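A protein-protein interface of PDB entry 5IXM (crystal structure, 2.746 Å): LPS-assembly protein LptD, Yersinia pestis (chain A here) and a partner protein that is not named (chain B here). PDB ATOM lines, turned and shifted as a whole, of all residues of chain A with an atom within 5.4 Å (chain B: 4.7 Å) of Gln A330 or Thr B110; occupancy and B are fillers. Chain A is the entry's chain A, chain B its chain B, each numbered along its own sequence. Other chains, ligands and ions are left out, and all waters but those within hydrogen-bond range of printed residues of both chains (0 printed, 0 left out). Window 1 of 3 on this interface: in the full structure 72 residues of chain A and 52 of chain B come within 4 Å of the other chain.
NE2 of Gln A330 is in hydrogen-bond range of O of Thr B110. The backbone NH (N) of Gln A330 sits at hydrogen-bond distance from the side-chain carboxylate (OE2) of Glu B124, at 3.3 Å. The guanidinium group (NE) of Arg A452 lies within salt-bridge range of the side-chain carboxylate (OE1) of Glu B82.
The backbone carbonyl oxygen (O) of Gln A330 lies within hydrogen-bond range of the guanidinium group (NH2) of Arg A338 (2.9 Å). The backbone carbonyl oxygen of Leu A432 sits at hydrogen-bond distance from the backbone NH of Gln A422 (2.8 Å). N of Asn B83 sits at hydrogen-bond distance from O of Phe B111, 2.9 Å away.
Among the printed residues, merely in contact across the chains: Arg A452 with Thr B110 (3.3 Å), Gln A330 with Phe B111 (3.3 Å), Tyr A458 with Phe B112 (3.5 Å), Gln A330 with Phe B112 (3.5 Å), Met A329 with Glu B124 (3.6 Å), Leu A432 with Glu B82 (3.6 Å) and Leu A432 with Phe B112 (3.7 Å).
Of chain A, only Gln A330 (3.1 Å) and Arg A452 (3.3 Å) come within 4 Å of Thr B110. Printed residues of chain B within 4 Å of Arg A452: Glu B82 (2.4 Å) and Thr B110 (3.3 Å). Printed residues of chain A within 4 Å of Glu B124: Met A329 and Gln A330. Of the printed residues of chain B, Tyr A458 touches Phe B112. Of the printed residues of chain A, Phe B111 touches Gln A330. Phe B108 touches none of the printed residues of chain A. The nearest printed residue of chain B that does not touch Gln A330 is Glu B82 (5.7 Å). The nearest printed residue of chain B that does not touch Tyr A458 is Glu B82 (6.8 Å).
Of the 10 printed residues of chain A, 5 touch a printed residue of chain B. Printed residues of chain A that touch a printed residue of chain B: Met A329, Gln A330, Leu A432, Arg A452 and Tyr A458. Hydrophobic or aromatic side chains of chain A within 4 Å of the printed part of chain B: Met A329, Leu A432 and Tyr A458. Along chain A the printed residues that touch a printed residue of chain B span positions 329 to 458. Of the 9 printed residues of chain B, 5 touch a printed residue of chain A. Printed residues of chain B that touch a printed residue of chain A: Glu B82, Thr B110, Phe B111, Phe B112 and Glu B124. Among the printed residues, 10 pairs touch across the chains.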
ATOM      1  N   LEU A 328      18.857  17.683  33.063  1.00  0.00           N
ATOM      2  CA  LEU A 328      19.557  16.411  33.036  1.00  0.00           C
ATOM      3  C   LEU A 328      21.011  16.655  32.662  1.00  0.00           C
ATOM      4  O   LEU A 328      21.296  17.213  31.602  1.00  0.00           O
ATOM      5  CB  LEU A 328      18.899  15.452  32.043  1.00  0.00           C
ATOM      6  CG  LEU A 328      19.505  14.053  31.935  1.00  0.00           C
ATOM      7  CD1 LEU A 328      19.509  13.376  33.292  1.00  0.00           C
ATOM      8  CD2 LEU A 328      18.749  13.212  30.914  1.00  0.00           C
ATOM      9  N   MET A 329      21.928  16.247  33.534  1.00  0.00           N
ATOM     10  CA  MET A 329      23.345  16.398  33.240  1.00  0.00           C
ATOM     11  C   MET A 329      23.690  15.422  32.135  1.00  0.00           C
ATOM     12  O   MET A 329      23.104  14.342  32.054  1.00  0.00           O
ATOM     13  CB  MET A 329      24.209  16.133  34.475  1.00  0.00           C
ATOM     14  CG  MET A 329      24.064  17.146  35.596  1.00  0.00           C
ATOM     15  SD  MET A 329      25.025  18.635  35.279  1.00  0.00           S
ATOM     16  CE  MET A 329      26.565  17.910  34.722  1.00  0.00           C
ATOM     17  N   GLN A 330      24.633  15.796  31.281  1.00  0.00           N
ATOM     18  CA  GLN A 330      25.059  14.890  30.229  1.00  0.00           C
ATOM     19  C   GLN A 330      26.282  14.103  30.663  1.00  0.00           C
ATOM     20  O   GLN A 330      27.307  14.674  31.039  1.00  0.00           O
ATOM     21  CB  GLN A 330      25.340  15.645  28.932  1.00  0.00           C
ATOM     22  CG  GLN A 330      25.912  14.757  27.841  1.00  0.00           C
ATOM     23  CD  GLN A 330      26.098  15.486  26.531  1.00  0.00           C
ATOM     24  OE1 GLN A 330      25.343  16.402  26.207  1.00  0.00           O
ATOM     25  NE2 GLN A 330      27.112  15.090  25.769  1.00  0.00           N
ATOM     26  N   SER A 331      26.155  12.783  30.604  1.00  0.00           N
ATOM     27  CA  SER A 331      27.213  11.881  31.029  1.00  0.00           C
ATOM     28  C   SER A 331      28.062  11.369  29.872  1.00  0.00           C
ATOM     29  O   SER A 331      27.546  10.802  28.914  1.00  0.00           O
ATOM     30  CB  SER A 331      26.613  10.689  31.778  1.00  0.00           C
ATOM     31  OG  SER A 331      25.560  10.101  31.032  1.00  0.00           O
ATOM     32  N   ASP A 332      29.370  11.558  29.982  1.00  0.00           N
ATOM     33  CA  ASP A 332      30.323  10.964  29.056  1.00  0.00           C
ATOM     34  C   ASP A 332      30.987   9.836  29.838  1.00  0.00           C
ATOM     35  O   ASP A 332      30.402   9.359  30.812  1.00  0.00           O
ATOM     36  CB  ASP A 332      31.331  11.991  28.542  1.00  0.00           C
ATOM     37  CG  ASP A 332      32.263  12.490  29.625  1.00  0.00           C
ATOM     38  OD1 ASP A 332      31.779  12.813  30.732  1.00  0.00           O
ATOM     39  OD2 ASP A 332      33.482  12.564  29.364  1.00  0.00           O
ATOM     40  N   ARG A 338      30.129  10.186  38.233  1.00  0.00           N
ATOM     41  CA  ARG A 338      29.534  11.364  38.855  1.00  0.00           C
ATOM     42  C   ARG A 338      28.362  10.945  39.741  1.00  0.00           C
ATOM     43  O   ARG A 338      27.532  10.130  39.338  1.00  0.00           O
ATOM     44  CB  ARG A 338      29.073  12.363  37.788  1.00  0.00           C
ATOM     45  CG  ARG A 338      28.382  13.594  38.352  1.00  0.00           C
ATOM     46  CD  ARG A 338      28.290  14.706  37.321  1.00  0.00           C
ATOM     47  NE  ARG A 338      27.591  14.283  36.111  1.00  0.00           N
ATOM     48  CZ  ARG A 338      28.074  14.411  34.879  1.00  0.00           C
ATOM     49  NH1 ARG A 338      29.275  14.936  34.683  1.00  0.00           N
ATOM     50  NH2 ARG A 338      27.356  14.000  33.844  1.00  0.00           N
ATOM     51  N   GLN A 422      28.327   6.679  23.581  1.00  0.00           N
ATOM     52  CA  GLN A 422      27.494   6.474  24.761  1.00  0.00           C
ATOM     53  C   GLN A 422      26.267   5.629  24.444  1.00  0.00           C
ATOM     54  O   GLN A 422      25.632   5.804  23.402  1.00  0.00           O
ATOM     55  CB  GLN A 422      27.055   7.820  25.337  1.00  0.00           C
ATOM     56  CG  GLN A 422      28.197   8.766  25.653  1.00  0.00           C
ATOM     57  CD  GLN A 422      27.710  10.139  26.054  1.00  0.00           C
ATOM     58  OE1 GLN A 422      26.538  10.322  26.388  1.00  0.00           O
ATOM     59  NE2 GLN A 422      28.606  11.118  26.019  1.00  0.00           N
ATOM     60  N   LEU A 432      24.772   8.923  21.900  1.00  0.00           N
ATOM     61  CA  LEU A 432      25.716   9.949  21.482  1.00  0.00           C
ATOM     62  C   LEU A 432      26.971   9.282  20.960  1.00  0.00           C
ATOM     63  O   LEU A 432      27.363   8.220  21.440  1.00  0.00           O
ATOM     64  CB  LEU A 432      26.067  10.882  22.646  1.00  0.00           C
ATOM     65  CG  LEU A 432      25.155  12.056  23.009  1.00  0.00           C
ATOM     66  CD1 LEU A 432      25.566  12.631  24.343  1.00  0.00           C
ATOM     67  CD2 LEU A 432      25.248  13.126  21.954  1.00  0.00           C
ATOM     68  N   ARG A 452      29.816  13.955  14.207  1.00  0.00           N
ATOM     69  CA  ARG A 452      29.044  14.032  15.434  1.00  0.00           C
ATOM     70  C   ARG A 452      27.674  13.408  15.229  1.00  0.00           C
ATOM     71  O   ARG A 452      26.996  13.676  14.243  1.00  0.00           O
ATOM     72  CB  ARG A 452      28.906  15.482  15.907  1.00  0.00           C
ATOM     73  CG  ARG A 452      30.231  16.210  16.058  1.00  0.00           C
ATOM     74  CD  ARG A 452      30.074  17.466  16.892  1.00  0.00           C
ATOM     75  NE  ARG A 452      29.482  17.152  18.187  1.00  0.00           N
ATOM     76  CZ  ARG A 452      30.181  16.806  19.264  1.00  0.00           C
ATOM     77  NH1 ARG A 452      31.504  16.733  19.205  1.00  0.00           N
ATOM     78  NH2 ARG A 452      29.557  16.532  20.400  1.00  0.00           N
ATOM     79  N   TYR A 458      17.603  10.528  22.409  1.00  0.00           N
ATOM     80  CA  TYR A 458      18.486  11.120  23.401  1.00  0.00           C
ATOM     81  C   TYR A 458      18.210  12.607  23.531  1.00  0.00           C
ATOM     82  O   TYR A 458      18.256  13.149  24.626  1.00  0.00           O
ATOM     83  CB  TYR A 458      19.967  10.917  23.082  1.00  0.00           C
ATOM     84  CG  TYR A 458      20.811  11.599  24.132  1.00  0.00           C
ATOM     85  CD1 TYR A 458      21.006  11.008  25.370  1.00  0.00           C
ATOM     86  CD2 TYR A 458      21.360  12.857  23.911  1.00  0.00           C
ATOM     87  CE1 TYR A 458      21.746  11.633  26.348  1.00  0.00           C
ATOM     88  CE2 TYR A 458      22.101  13.492  24.886  1.00  0.00           C
ATOM     89  CZ  TYR A 458      22.292  12.874  26.104  1.00  0.00           C
ATOM     90  OH  TYR A 458      23.032  13.493  27.084  1.00  0.00           O
ATOM     91  N   GLU B  82      24.853  21.377  19.985  1.00  0.00           N
ATOM     92  CA  GLU B  82      25.844  21.016  20.987  1.00  0.00           C
ATOM     93  C   GLU B  82      26.849  22.142  21.158  1.00  0.00           C
ATOM     94  O   GLU B  82      27.303  22.738  20.179  1.00  0.00           O
ATOM     95  CB  GLU B  82      26.584  19.734  20.599  1.00  0.00           C
ATOM     96  CG  GLU B  82      25.731  18.482  20.523  1.00  0.00           C
ATOM     97  CD  GLU B  82      26.454  17.339  19.824  1.00  0.00           C
ATOM     98  OE1 GLU B  82      27.180  17.605  18.842  1.00  0.00           O
ATOM     99  OE2 GLU B  82      26.303  16.177  20.259  1.00  0.00           O
ATOM    100  N   ASN B  83      27.190  22.429  22.409  1.00  0.00           N
ATOM    101  CA  ASN B  83      28.248  23.376  22.721  1.00  0.00           C
ATOM    102  C   ASN B  83      29.416  22.666  23.388  1.00  0.00           C
ATOM    103  O   ASN B  83      29.233  21.658  24.088  1.00  0.00           O
ATOM    104  CB  ASN B  83      27.724  24.504  23.611  1.00  0.00           C
ATOM    105  CG  ASN B  83      26.777  25.433  22.875  1.00  0.00           C
ATOM    106  OD1 ASN B  83      27.039  25.830  21.740  1.00  0.00           O
ATOM    107  ND2 ASN B  83      25.671  25.785  23.519  1.00  0.00           N
ATOM    108  N   GLN B  84      30.617  23.191  23.162  1.00  0.00           N
ATOM    109  CA  GLN B  84      31.828  22.596  23.708  1.00  0.00           C
ATOM    110  C   GLN B  84      32.602  23.559  24.604  1.00  0.00           C
ATOM    111  O   GLN B  84      32.952  24.666  24.195  1.00  0.00           O
ATOM    112  CB  GLN B  84      32.733  22.095  22.582  1.00  0.00           C
ATOM    113  CG  GLN B  84      34.026  21.479  23.078  1.00  0.00           C
ATOM    114  CD  GLN B  84      34.868  20.905  21.963  1.00  0.00           C
ATOM    115  OE1 GLN B  84      34.958  19.687  21.803  1.00  0.00           O
ATOM    116  NE2 GLN B  84      35.477  21.778  21.171  1.00  0.00           N
ATOM    117  N   PHE B 108      38.283  18.936  27.282  1.00  0.00           N
ATOM    118  CA  PHE B 108      37.087  19.230  26.493  1.00  0.00           C
ATOM    119  C   PHE B 108      35.825  18.593  27.076  1.00  0.00           C
ATOM    120  O   PHE B 108      35.860  17.464  27.563  1.00  0.00           O
ATOM    121  CB  PHE B 108      37.278  18.751  25.050  1.00  0.00           C
ATOM    122  CG  PHE B 108      38.466  19.360  24.356  1.00  0.00           C
ATOM    123  CD1 PHE B 108      39.730  18.816  24.508  1.00  0.00           C
ATOM    124  CD2 PHE B 108      38.313  20.471  23.542  1.00  0.00           C
ATOM    125  CE1 PHE B 108      40.823  19.377  23.873  1.00  0.00           C
ATOM    126  CE2 PHE B 108      39.402  21.034  22.902  1.00  0.00           C
ATOM    127  CZ  PHE B 108      40.658  20.485  23.066  1.00  0.00           C
ATOM    128  N   ARG B 109      34.713  19.319  27.023  1.00  0.00           N
ATOM    129  CA  ARG B 109      33.412  18.736  27.363  1.00  0.00           C
ATOM    130  C   ARG B 109      32.345  19.215  26.388  1.00  0.00           C
ATOM    131  O   ARG B 109      32.497  20.260  25.764  1.00  0.00           O
ATOM    132  CB  ARG B 109      32.993  19.091  28.791  1.00  0.00           C
ATOM    133  CG  ARG B 109      33.736  18.365  29.898  1.00  0.00           C
ATOM    134  CD  ARG B 109      33.433  16.876  29.927  1.00  0.00           C
ATOM    135  NE  ARG B 109      33.983  16.229  31.117  1.00  0.00           N
ATOM    136  CZ  ARG B 109      35.275  15.988  31.318  1.00  0.00           C
ATOM    137  NH1 ARG B 109      36.171  16.335  30.403  1.00  0.00           N
ATOM    138  NH2 ARG B 109      35.673  15.394  32.437  1.00  0.00           N
ATOM    139  N   THR B 110      31.260  18.456  26.270  1.00  0.00           N
ATOM    140  CA  THR B 110      30.183  18.800  25.347  1.00  0.00           C
ATOM    141  C   THR B 110      28.814  18.654  26.006  1.00  0.00           C
ATOM    142  O   THR B 110      28.565  17.684  26.719  1.00  0.00           O
ATOM    143  CB  THR B 110      30.240  17.914  24.081  1.00  0.00           C
ATOM    144  OG1 THR B 110      31.402  18.250  23.312  1.00  0.00           O
ATOM    145  CG2 THR B 110      29.001  18.102  23.224  1.00  0.00           C
ATOM    146  N   PHE B 111      27.924  19.615  25.769  1.00  0.00           N
ATOM    147  CA  PHE B 111      26.556  19.492  26.269  1.00  0.00           C
ATOM    148  C   PHE B 111      25.580  20.188  25.331  1.00  0.00           C
ATOM    149  O   PHE B 111      25.947  21.134  24.645  1.00  0.00           O
ATOM    150  CB  PHE B 111      26.441  20.065  27.683  1.00  0.00           C
ATOM    151  CG  PHE B 111      26.615  21.554  27.754  1.00  0.00           C
ATOM    152  CD1 PHE B 111      27.871  22.129  27.653  1.00  0.00           C
ATOM    153  CD2 PHE B 111      25.520  22.378  27.952  1.00  0.00           C
ATOM    154  CE1 PHE B 111      28.029  23.502  27.726  1.00  0.00           C
ATOM    155  CE2 PHE B 111      25.671  23.750  28.032  1.00  0.00           C
ATOM    156  CZ  PHE B 111      26.926  24.313  27.918  1.00  0.00           C
ATOM    157  N   PHE B 112      24.337  19.720  25.304  1.00  0.00           N
ATOM    158  CA  PHE B 112      23.310  20.352  24.486  1.00  0.00           C
ATOM    159  C   PHE B 112      22.844  21.658  25.109  1.00  0.00           C
ATOM    160  O   PHE B 112      22.825  21.800  26.331  1.00  0.00           O
ATOM    161  CB  PHE B 112      22.120  19.412  24.292  1.00  0.00           C
ATOM    162  CG  PHE B 112      22.387  18.299  23.322  1.00  0.00           C
ATOM    163  CD1 PHE B 112      22.958  17.114  23.749  1.00  0.00           C
ATOM    164  CD2 PHE B 112      22.082  18.445  21.978  1.00  0.00           C
ATOM    165  CE1 PHE B 112      23.210  16.093  22.860  1.00  0.00           C
ATOM    166  CE2 PHE B 112      22.331  17.427  21.085  1.00  0.00           C
ATOM    167  CZ  PHE B 112      22.897  16.250  21.528  1.00  0.00           C
ATOM    168  N   GLU B 124      24.665  23.552  34.882  1.00  0.00           N
ATOM    169  CA  GLU B 124      25.331  22.399  34.291  1.00  0.00           C
ATOM    170  C   GLU B 124      26.757  22.769  33.905  1.00  0.00           C
ATOM    171  O   GLU B 124      27.711  22.065  34.259  1.00  0.00           O
ATOM    172  CB  GLU B 124      24.564  21.887  33.070  1.00  0.00           C
ATOM    173  CG  GLU B 124      25.224  20.708  32.373  1.00  0.00           C
ATOM    174  CD  GLU B 124      24.401  20.168  31.217  1.00  0.00           C
ATOM    175  OE1 GLU B 124      23.408  20.822  30.828  1.00  0.00           O
ATOM    176  OE2 GLU B 124      24.743  19.085  30.698  1.00  0.00           O
